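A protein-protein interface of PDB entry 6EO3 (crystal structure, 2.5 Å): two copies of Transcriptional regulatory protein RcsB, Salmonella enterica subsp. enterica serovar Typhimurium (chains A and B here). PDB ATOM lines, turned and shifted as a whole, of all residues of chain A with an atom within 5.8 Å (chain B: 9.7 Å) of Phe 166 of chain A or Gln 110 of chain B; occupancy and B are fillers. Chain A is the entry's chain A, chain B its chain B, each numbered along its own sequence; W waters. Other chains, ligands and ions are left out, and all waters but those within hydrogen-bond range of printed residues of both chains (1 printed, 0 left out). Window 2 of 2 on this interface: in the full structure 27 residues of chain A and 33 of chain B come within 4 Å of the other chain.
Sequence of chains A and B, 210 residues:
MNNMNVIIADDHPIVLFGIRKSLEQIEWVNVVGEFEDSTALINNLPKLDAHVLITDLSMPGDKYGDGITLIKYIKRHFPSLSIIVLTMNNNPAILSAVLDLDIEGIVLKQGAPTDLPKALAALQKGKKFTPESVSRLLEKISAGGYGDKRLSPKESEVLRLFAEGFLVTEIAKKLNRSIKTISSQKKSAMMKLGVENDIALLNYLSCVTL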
ATOM      1  N   LEU A 161       5.336 -20.987  11.305  1.00  0.00           N
ATOM      2  CA  LEU A 161       6.038 -19.856  10.720  1.00  0.00           C
ATOM      3  C   LEU A 161       5.876 -19.838   9.207  1.00  0.00           C
ATOM      4  O   LEU A 161       5.650 -18.782   8.612  1.00  0.00           O
ATOM      5  CB  LEU A 161       7.516 -19.904  11.100  1.00  0.00           C
ATOM      6  CG  LEU A 161       7.815 -19.727  12.593  1.00  0.00           C
ATOM      7  CD1 LEU A 161       9.295 -19.951  12.868  1.00  0.00           C
ATOM      8  CD2 LEU A 161       7.379 -18.363  13.113  1.00  0.00           C
ATOM      9  N   PHE A 162       5.965 -21.008   8.582  1.00  0.00           N
ATOM     10  CA  PHE A 162       5.772 -21.093   7.143  1.00  0.00           C
ATOM     11  C   PHE A 162       4.360 -20.633   6.737  1.00  0.00           C
ATOM     12  O   PHE A 162       4.195 -19.905   5.748  1.00  0.00           O
ATOM     13  CB  PHE A 162       6.030 -22.509   6.646  1.00  0.00           C
ATOM     14  CG  PHE A 162       6.114 -22.601   5.145  1.00  0.00           C
ATOM     15  CD1 PHE A 162       7.190 -22.038   4.468  1.00  0.00           C
ATOM     16  CD2 PHE A 162       5.111 -23.215   4.408  1.00  0.00           C
ATOM     17  CE1 PHE A 162       7.268 -22.094   3.086  1.00  0.00           C
ATOM     18  CE2 PHE A 162       5.186 -23.268   3.030  1.00  0.00           C
ATOM     19  CZ  PHE A 162       6.267 -22.704   2.367  1.00  0.00           C
ATOM     20  N   ALA A 163       3.356 -21.051   7.515  1.00  0.00           N
ATOM     21  CA  ALA A 163       1.958 -20.666   7.294  1.00  0.00           C
ATOM     22  C   ALA A 163       1.782 -19.167   7.369  1.00  0.00           C
ATOM     23  O   ALA A 163       0.952 -18.604   6.674  1.00  0.00           O
ATOM     24  CB  ALA A 163       1.044 -21.333   8.316  1.00  0.00           C
ATOM     25  N   GLU A 164       2.564 -18.524   8.226  1.00  0.00           N
ATOM     26  CA  GLU A 164       2.490 -17.085   8.394  1.00  0.00           C
ATOM     27  C   GLU A 164       3.290 -16.340   7.326  1.00  0.00           C
ATOM     28  O   GLU A 164       3.443 -15.126   7.399  1.00  0.00           O
ATOM     29  CB  GLU A 164       2.960 -16.728   9.797  1.00  0.00           C
ATOM     30  CG  GLU A 164       2.046 -17.301  10.868  1.00  0.00           C
ATOM     31  CD  GLU A 164       2.446 -16.911  12.274  1.00  0.00           C
ATOM     32  OE1 GLU A 164       3.662 -16.896  12.582  1.00  0.00           O
ATOM     33  OE2 GLU A 164       1.531 -16.626  13.072  1.00  0.00           O
ATOM     34  N   GLY A 165       3.795 -17.072   6.340  1.00  0.00           N
ATOM     35  CA  GLY A 165       4.441 -16.479   5.173  1.00  0.00           C
ATOM     36  C   GLY A 165       5.918 -16.186   5.331  1.00  0.00           C
ATOM     37  O   GLY A 165       6.469 -15.331   4.634  1.00  0.00           O
ATOM     38  N   PHE A 166       6.569 -16.883   6.252  1.00  0.00           N
ATOM     39  CA  PHE A 166       8.014 -16.818   6.328  1.00  0.00           C
ATOM     40  C   PHE A 166       8.611 -17.794   5.315  1.00  0.00           C
ATOM     41  O   PHE A 166       8.126 -18.916   5.155  1.00  0.00           O
ATOM     42  CB  PHE A 166       8.508 -17.127   7.744  1.00  0.00           C
ATOM     43  CG  PHE A 166       8.287 -16.005   8.714  1.00  0.00           C
ATOM     44  CD1 PHE A 166       9.167 -14.940   8.766  1.00  0.00           C
ATOM     45  CD2 PHE A 166       7.192 -16.004   9.561  1.00  0.00           C
ATOM     46  CE1 PHE A 166       8.964 -13.896   9.650  1.00  0.00           C
ATOM     47  CE2 PHE A 166       6.978 -14.958  10.444  1.00  0.00           C
ATOM     48  CZ  PHE A 166       7.864 -13.903  10.487  1.00  0.00           C
ATOM     49  N   LEU A 167       9.652 -17.347   4.624  1.00  0.00           N
ATOM     50  CA  LEU A 167      10.426 -18.211   3.749  1.00  0.00           C
ATOM     51  C   LEU A 167      11.303 -19.087   4.621  1.00  0.00           C
ATOM     52  O   LEU A 167      11.589 -18.741   5.766  1.00  0.00           O
ATOM     53  CB  LEU A 167      11.291 -17.375   2.805  1.00  0.00           C
ATOM     54  CG  LEU A 167      10.527 -16.385   1.918  1.00  0.00           C
ATOM     55  CD1 LEU A 167      11.472 -15.399   1.235  1.00  0.00           C
ATOM     56  CD2 LEU A 167       9.686 -17.152   0.902  1.00  0.00           C
ATOM     57  N   VAL A 168      11.721 -20.227   4.087  1.00  0.00           N
ATOM     58  CA  VAL A 168      12.590 -21.145   4.834  1.00  0.00           C
ATOM     59  C   VAL A 168      13.907 -20.470   5.272  1.00  0.00           C
ATOM     60  O   VAL A 168      14.442 -20.786   6.334  1.00  0.00           O
ATOM     61  CB  VAL A 168      12.850 -22.471   4.071  1.00  0.00           C
ATOM     62  CG1 VAL A 168      11.574 -23.302   4.005  1.00  0.00           C
ATOM     63  CG2 VAL A 168      13.383 -22.220   2.664  1.00  0.00           C
ATOM     64  N   GLU A 170      14.172 -17.232   6.146  1.00  0.00           N
ATOM     65  CA  GLU A 170      13.786 -16.446   7.314  1.00  0.00           C
ATOM     66  C   GLU A 170      13.583 -17.341   8.531  1.00  0.00           C
ATOM     67  O   GLU A 170      14.013 -17.005   9.632  1.00  0.00           O
ATOM     68  CB  GLU A 170      12.501 -15.676   7.038  1.00  0.00           C
ATOM     69  CG  GLU A 170      12.654 -14.580   6.000  1.00  0.00           C
ATOM     70  CD  GLU A 170      11.315 -14.046   5.514  1.00  0.00           C
ATOM     71  OE1 GLU A 170      10.474 -14.858   5.069  1.00  0.00           O
ATOM     72  OE2 GLU A 170      11.108 -12.816   5.562  1.00  0.00           O
ATOM     73  N   ILE A 171      12.922 -18.477   8.322  1.00  0.00           N
ATOM     74  CA  ILE A 171      12.616 -19.407   9.411  1.00  0.00           C
ATOM     75  C   ILE A 171      13.907 -19.951  10.043  1.00  0.00           C
ATOM     76  O   ILE A 171      13.959 -20.197  11.247  1.00  0.00           O
ATOM     77  CB  ILE A 171      11.713 -20.561   8.929  1.00  0.00           C
ATOM     78  CG1 ILE A 171      10.339 -20.023   8.516  1.00  0.00           C
ATOM     79  CG2 ILE A 171      11.538 -21.603  10.031  1.00  0.00           C
ATOM     80  CD1 ILE A 171       9.438 -21.037   7.836  1.00  0.00           C
ATOM     81  N   LYS A 174      15.304 -17.142  12.372  1.00  0.00           N
ATOM     82  CA  LYS A 174      14.475 -16.942  13.565  1.00  0.00           C
ATOM     83  C   LYS A 174      14.614 -18.073  14.584  1.00  0.00           C
ATOM     84  O   LYS A 174      14.878 -17.824  15.757  1.00  0.00           O
ATOM     85  CB  LYS A 174      13.000 -16.757  13.193  1.00  0.00           C
ATOM     86  CG  LYS A 174      12.731 -15.542  12.317  1.00  0.00           C
ATOM     87  CD  LYS A 174      11.564 -14.706  12.835  1.00  0.00           C
ATOM     88  CE  LYS A 174      10.240 -15.456  12.787  1.00  0.00           C
ATOM     89  NZ  LYS A 174       9.173 -14.735  13.537  1.00  0.00           N
ATOM     90  N   LEU B  86      -5.489  -7.779   4.348  1.00  0.00           N
ATOM     91  CA  LEU B  86      -4.537  -7.974   5.423  1.00  0.00           C
ATOM     92  C   LEU B  86      -4.853  -9.304   6.087  1.00  0.00           C
ATOM     93  O   LEU B  86      -5.896  -9.438   6.715  1.00  0.00           O
ATOM     94  CB  LEU B  86      -4.689  -6.832   6.423  1.00  0.00           C
ATOM     95  CG  LEU B  86      -3.566  -6.554   7.417  1.00  0.00           C
ATOM     96  CD1 LEU B  86      -2.257  -6.210   6.719  1.00  0.00           C
ATOM     97  CD2 LEU B  86      -3.995  -5.409   8.318  1.00  0.00           C
ATOM     98  N   THR B  87      -3.961 -10.285   5.947  1.00  0.00           N
ATOM     99  CA  THR B  87      -4.214 -11.631   6.468  1.00  0.00           C
ATOM    100  C   THR B  87      -3.038 -12.218   7.260  1.00  0.00           C
ATOM    101  O   THR B  87      -1.882 -11.899   7.002  1.00  0.00           O
ATOM    102  CB  THR B  87      -4.595 -12.602   5.333  1.00  0.00           C
ATOM    103  OG1 THR B  87      -4.969 -13.870   5.889  1.00  0.00           O
ATOM    104  CG2 THR B  87      -3.437 -12.806   4.351  1.00  0.00           C
ATOM    105  N   MET B  88      -3.356 -13.074   8.229  1.00  0.00           N
ATOM    106  CA  MET B  88      -2.345 -13.716   9.079  1.00  0.00           C
ATOM    107  C   MET B  88      -1.632 -14.858   8.355  1.00  0.00           C
ATOM    108  O   MET B  88      -0.415 -15.023   8.475  1.00  0.00           O
ATOM    109  CB  MET B  88      -2.977 -14.253  10.375  1.00  0.00           C
ATOM    110  CG  MET B  88      -1.978 -14.827  11.383  1.00  0.00           C
ATOM    111  SD  MET B  88      -0.831 -13.628  12.112  1.00  0.00           S
ATOM    112  CE  MET B  88      -1.936 -12.766  13.233  1.00  0.00           C
ATOM    113  N   ASN B  89      -2.396 -15.653   7.618  1.00  0.00           N
ATOM    114  CA  ASN B  89      -1.866 -16.865   7.018  1.00  0.00           C
ATOM    115  C   ASN B  89      -1.754 -16.777   5.500  1.00  0.00           C
ATOM    116  O   ASN B  89      -2.412 -15.970   4.839  1.00  0.00           O
ATOM    117  CB  ASN B  89      -2.719 -18.064   7.442  1.00  0.00           C
ATOM    118  CG  ASN B  89      -2.775 -18.232   8.955  1.00  0.00           C
ATOM    119  OD1 ASN B  89      -3.815 -18.012   9.570  1.00  0.00           O
ATOM    120  ND2 ASN B  89      -1.646 -18.586   9.563  1.00  0.00           N
ATOM    121  N   ASN B  90      -0.877 -17.607   4.963  1.00  0.00           N
ATOM    122  CA  ASN B  90      -0.723 -17.757   3.533  1.00  0.00           C
ATOM    123  C   ASN B  90      -1.738 -18.832   3.172  1.00  0.00           C
ATOM    124  O   ASN B  90      -1.535 -20.008   3.484  1.00  0.00           O
ATOM    125  CB  ASN B  90       0.714 -18.193   3.215  1.00  0.00           C
ATOM    126  CG  ASN B  90       1.263 -17.575   1.943  1.00  0.00           C
ATOM    127  OD1 ASN B  90       0.542 -16.948   1.174  1.00  0.00           O
ATOM    128  ND2 ASN B  90       2.559 -17.756   1.720  1.00  0.00           N
ATOM    129  N   VAL B 107      -1.291  -8.300   2.074  1.00  0.00           N
ATOM    130  CA  VAL B 107      -0.246  -8.105   3.077  1.00  0.00           C
ATOM    131  C   VAL B 107      -0.411  -9.088   4.240  1.00  0.00           C
ATOM    132  O   VAL B 107      -1.477  -9.195   4.865  1.00  0.00           O
ATOM    133  CB  VAL B 107      -0.226  -6.653   3.608  1.00  0.00           C
ATOM    134  CG1 VAL B 107       0.859  -6.481   4.671  1.00  0.00           C
ATOM    135  CG2 VAL B 107      -0.015  -5.667   2.465  1.00  0.00           C
ATOM    136  N   LEU B 108       0.664  -9.798   4.533  1.00  0.00           N
ATOM    137  CA  LEU B 108       0.678 -10.722   5.653  1.00  0.00           C
ATOM    138  C   LEU B 108       0.903  -9.953   6.954  1.00  0.00           C
ATOM    139  O   LEU B 108       1.738  -9.050   7.014  1.00  0.00           O
ATOM    140  CB  LEU B 108       1.760 -11.773   5.441  1.00  0.00           C
ATOM    141  CG  LEU B 108       1.518 -12.679   4.229  1.00  0.00           C
ATOM    142  CD1 LEU B 108       2.720 -13.565   4.020  1.00  0.00           C
ATOM    143  CD2 LEU B 108       0.265 -13.528   4.384  1.00  0.00           C
ATOM    144  N   LYS B 109       0.159 -10.319   7.992  1.00  0.00           N
ATOM    145  CA  LYS B 109       0.166  -9.564   9.250  1.00  0.00           C
ATOM    146  C   LYS B 109       1.527  -9.536   9.935  1.00  0.00           C
ATOM    147  O   LYS B 109       1.855  -8.572  10.620  1.00  0.00           O
ATOM    148  CB  LYS B 109      -0.907 -10.087  10.204  1.00  0.00           C
ATOM    149  CG  LYS B 109      -2.306  -9.723   9.739  1.00  0.00           C
ATOM    150  CD  LYS B 109      -3.382 -10.078  10.744  1.00  0.00           C
ATOM    151  CE  LYS B 109      -4.760  -9.760  10.184  1.00  0.00           C
ATOM    152  NZ  LYS B 109      -5.771  -9.720  11.273  1.00  0.00           N
ATOM    153  N   GLN B 110       2.321 -10.581   9.743  1.00  0.00           N
ATOM    154  CA  GLN B 110       3.639 -10.620  10.355  1.00  0.00           C
ATOM    155  C   GLN B 110       4.530  -9.466   9.890  1.00  0.00           C
ATOM    156  O   GLN B 110       5.205  -8.850  10.698  1.00  0.00           O
ATOM    157  CB  GLN B 110       4.314 -11.963  10.112  1.00  0.00           C
ATOM    158  CG  GLN B 110       3.839 -13.050  11.059  1.00  0.00           C
ATOM    159  CD  GLN B 110       4.294 -12.843  12.503  1.00  0.00           C
ATOM    160  OE1 GLN B 110       5.163 -12.023  12.789  1.00  0.00           O
ATOM    161  NE2 GLN B 110       3.692 -13.586  13.419  1.00  0.00           N
ATOM    162  N   GLY B 111       4.516  -9.161   8.601  1.00  0.00           N
ATOM    163  CA  GLY B 111       5.336  -8.073   8.070  1.00  0.00           C
ATOM    164  C   GLY B 111       4.592  -6.772   7.816  1.00  0.00           C
ATOM    165  O   GLY B 111       5.072  -5.946   7.056  1.00  0.00           O
ATOM    166  N   ALA B 112       3.441  -6.580   8.459  1.00  0.00           N
ATOM    167  CA  ALA B 112       2.605  -5.394   8.219  1.00  0.00           C
ATOM    168  C   ALA B 112       3.320  -4.052   8.443  1.00  0.00           C
ATOM    169  O   ALA B 112       3.263  -3.189   7.577  1.00  0.00           O
ATOM    170  CB  ALA B 112       1.329  -5.457   9.048  1.00  0.00           C
ATOM    171  N   PRO B 113       3.989  -3.866   9.598  1.00  0.00           N
ATOM    172  CA  PRO B 113       4.708  -2.598   9.829  1.00  0.00           C
ATOM    173  C   PRO B 113       5.669  -2.178   8.706  1.00  0.00           C
ATOM    174  O   PRO B 113       5.760  -0.993   8.377  1.00  0.00           O
ATOM    175  CB  PRO B 113       5.497  -2.865  11.121  1.00  0.00           C
ATOM    176  CG  PRO B 113       5.209  -4.275  11.522  1.00  0.00           C
ATOM    177  CD  PRO B 113       3.971  -4.700  10.810  1.00  0.00           C
ATOM    178  N   THR B 114       6.373  -3.154   8.141  1.00  0.00           N
ATOM    179  CA  THR B 114       7.319  -2.938   7.050  1.00  0.00           C
ATOM    180  C   THR B 114       6.635  -2.829   5.689  1.00  0.00           C
ATOM    181  O   THR B 114       6.998  -1.985   4.874  1.00  0.00           O
ATOM    182  CB  THR B 114       8.299  -4.120   6.960  1.00  0.00           C
ATOM    183  OG1 THR B 114       8.898  -4.341   8.239  1.00  0.00           O
ATOM    184  CG2 THR B 114       9.391  -3.865   5.928  1.00  0.00           C
ATOM    185  N   ASP B 115       5.658  -3.698   5.455  1.00  0.00           N
ATOM    186  CA  ASP B 115       5.107  -3.911   4.122  1.00  0.00           C
ATOM    187  C   ASP B 115       3.921  -3.023   3.799  1.00  0.00           C
ATOM    188  O   ASP B 115       3.634  -2.776   2.632  1.00  0.00           O
ATOM    189  CB  ASP B 115       4.697  -5.373   3.943  1.00  0.00           C
ATOM    190  CG  ASP B 115       5.885  -6.291   3.706  1.00  0.00           C
ATOM    191  OD1 ASP B 115       7.047  -5.816   3.665  1.00  0.00           O
ATOM    192  OD2 ASP B 115       5.647  -7.505   3.551  1.00  0.00           O
ATOM    193  N   LEU B 116       3.223  -2.552   4.821  1.00  0.00           N
ATOM    194  CA  LEU B 116       2.040  -1.721   4.593  1.00  0.00           C
ATOM    195  C   LEU B 116       2.413  -0.404   3.888  1.00  0.00           C
ATOM    196  O   LEU B 116       1.763  -0.019   2.918  1.00  0.00           O
ATOM    197  CB  LEU B 116       1.287  -1.468   5.905  1.00  0.00           C
ATOM    198  CG  LEU B 116      -0.223  -1.732   5.952  1.00  0.00           C
ATOM    199  CD1 LEU B 116      -0.668  -2.995   5.226  1.00  0.00           C
ATOM    200  CD2 LEU B 116      -0.660  -1.807   7.409  1.00  0.00           C
ATOM    201  N   PRO B 131       3.892 -10.107  -1.213  1.00  0.00           N
ATOM    202  CA  PRO B 131       5.241 -10.488  -0.786  1.00  0.00           C
ATOM    203  C   PRO B 131       5.675 -11.789  -1.438  1.00  0.00           C
ATOM    204  O   PRO B 131       4.827 -12.556  -1.906  1.00  0.00           O
ATOM    205  CB  PRO B 131       5.104 -10.642   0.734  1.00  0.00           C
ATOM    206  CG  PRO B 131       3.663 -10.958   0.966  1.00  0.00           C
ATOM    207  CD  PRO B 131       2.885 -10.332  -0.159  1.00  0.00           C
ATOM    208  N   GLU B 132       6.987 -12.022  -1.470  1.00  0.00           N
ATOM    209  CA  GLU B 132       7.557 -13.228  -2.081  1.00  0.00           C
ATOM    210  C   GLU B 132       6.799 -14.509  -1.719  1.00  0.00           C
ATOM    211  O   GLU B 132       6.424 -15.300  -2.593  1.00  0.00           O
ATOM    212  CB  GLU B 132       9.030 -13.383  -1.690  1.00  0.00           C
ATOM    213  CG  GLU B 132      10.013 -12.950  -2.768  1.00  0.00           C
ATOM    214  CD  GLU B 132       9.941 -13.821  -4.012  1.00  0.00           C
ATOM    215  OE1 GLU B 132       9.440 -14.965  -3.920  1.00  0.00           O
ATOM    216  OE2 GLU B 132      10.386 -13.355  -5.083  1.00  0.00           O
ATOM    217  N   SER B 133       6.581 -14.707  -0.424  1.00  0.00           N
ATOM    218  CA  SER B 133       5.870 -15.889   0.070  1.00  0.00           C
ATOM    219  C   SER B 133       4.568 -16.088  -0.687  1.00  0.00           C
ATOM    220  O   SER B 133       4.226 -17.208  -1.042  1.00  0.00           O
ATOM    221  CB  SER B 133       5.585 -15.761   1.557  1.00  0.00           C
ATOM    222  N   VAL B 134       3.845 -14.996  -0.928  1.00  0.00           N
ATOM    223  CA  VAL B 134       2.559 -15.060  -1.608  1.00  0.00           C
ATOM    224  C   VAL B 134       2.739 -15.261  -3.115  1.00  0.00           C
ATOM    225  O   VAL B 134       2.268 -16.258  -3.668  1.00  0.00           O
ATOM    226  CB  VAL B 134       1.719 -13.805  -1.312  1.00  0.00           C
ATOM    227  CG1 VAL B 134       0.413 -13.824  -2.092  1.00  0.00           C
ATOM    228  CG2 VAL B 134       1.426 -13.721   0.174  1.00  0.00           C
ATOM    229  N   ARG B 136       5.019 -16.440  -4.941  1.00  0.00           N
ATOM    230  CA  ARG B 136       5.500 -17.783  -5.316  1.00  0.00           C
ATOM    231  C   ARG B 136       4.361 -18.783  -5.435  1.00  0.00           C
ATOM    232  O   ARG B 136       4.366 -19.639  -6.311  1.00  0.00           O
ATOM    233  CB  ARG B 136       6.494 -18.321  -4.295  1.00  0.00           C
ATOM    234  CG  ARG B 136       7.914 -17.848  -4.499  1.00  0.00           C
ATOM    235  CD  ARG B 136       8.835 -18.549  -3.516  1.00  0.00           C
ATOM    236  NE  ARG B 136      10.079 -17.818  -3.299  1.00  0.00           N
ATOM    237  CZ  ARG B 136      11.070 -18.238  -2.516  1.00  0.00           C
ATOM    238  NH1 ARG B 136      10.979 -19.396  -1.865  1.00  0.00           N
ATOM    239  NH2 ARG B 136      12.160 -17.494  -2.382  1.00  0.00           N
HETATM  240  O   HOH W   1       1.729 -13.431   8.598  1.00  0.00           O
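NE2 of Gln 110 of chain B sits at hydrogen-bond distance from OE1 of Glu 164 of chain A (3.4 Å). The backbone carbonyl oxygen (O) of Ala 163 of chain A is in hydrogen-bond range of the backbone NH (N) of Asn 90 of chain B (2.7 Å).
Water W1 lies within hydrogen-bond range of the backbone carbonyl oxygen of Met 88 of chain B (2.7 Å), the backbone carbonyl oxygen of Glu 164 of chain A (2.7 Å) and the backbone NH of Gln 110 of chain B (3.1 Å).
Hydrophobic or aromatic side chains of chain A within 4 Å of the printed part of chain B: Phe 166 and Leu 167. Printed residues of chain B that touch a printed residue of chain A: Met 88, Asn 89, Asn 90, Leu 108, Gln 110, Ser 133 and Arg 136. Hydrophobic or aromatic side chains of chain B that line the printed part of chain A: Met 88 and Leu 108. Among the printed residues, 9 pairs touch across the chains. Among the printed residues, no Asp or Glu carboxylate lies within 4 Å of a Lys or Arg side-chain nitrogen of the other chain.
Of the printed residues of chain B, Gly 165 of chain A touches Leu 108 (3.6 Å) and Ser 133 (3.2 Å). Of chain B, only Gln 110 (3.7 Å) comes within 4 Å of Phe 166 of chain A. Leu 167 of chain A touches just one residue of chain B: Arg 136 (3.8 Å). Printed residues of chain A within 4 Å of Asn 89 of chain B: Ala 163. Printed residues of chain A within 4 Å of Asn 90 of chain B: Ala 163 (2.7 Å). Gln 110 of chain B touches two residues of chain A. Gly 111 of chain B touches none of the printed residues of chain A. Thr 114 of chain B touches none of the printed residues of chain A. Of the printed residues of chain A, Ser 133 of chain B touches Gly 165. Of the printed residues of chain A, Arg 136 of chain B touches Leu 167. The nearest printed residue of chain B that does not touch Ala 163 of chain A is Met 88 of chain B (4.2 Å).
The side-chain hydroxyl (OG1) of Thr 87 of chain B lies close to the backbone carbonyl oxygen (O) of Asn 89 of chain B. The side-chain amide nitrogen (ND2) of Asn 90 of chain B is in hydrogen-bond range of the backbone carbonyl oxygen (O) of Ser 133 of chain B (3.3 Å). OE1 of Glu 132 of chain B is in salt-bridge range of NE of Arg 136 of chain B (3.0 Å). The backbone NH of Phe 166 of chain A sits at hydrogen-bond distance from the backbone carbonyl oxygen of Leu 161 of chain A. The backbone NH (N) of Leu 167 of chain A sits at hydrogen-bond distance from the side-chain carboxylate (OE1) of Glu 170 of chain A (2.7 Å).
Among the printed residues, pairs that only touch across the chains: Gly 165 of chain A with Ser 133 of chain B, Ala 163 of chain A with Asn 89 of chain B, Glu 164 of chain A with Met 88 of chain B, Gly 165 of chain A with Leu 108 of chain B, Phe 166 of chain A with Gln 110 of chain B, Leu 167 of chain A with Arg 136 of chain B and Glu 164 of chain A with Leu 108 of chain B.
No position is printed for both chains.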
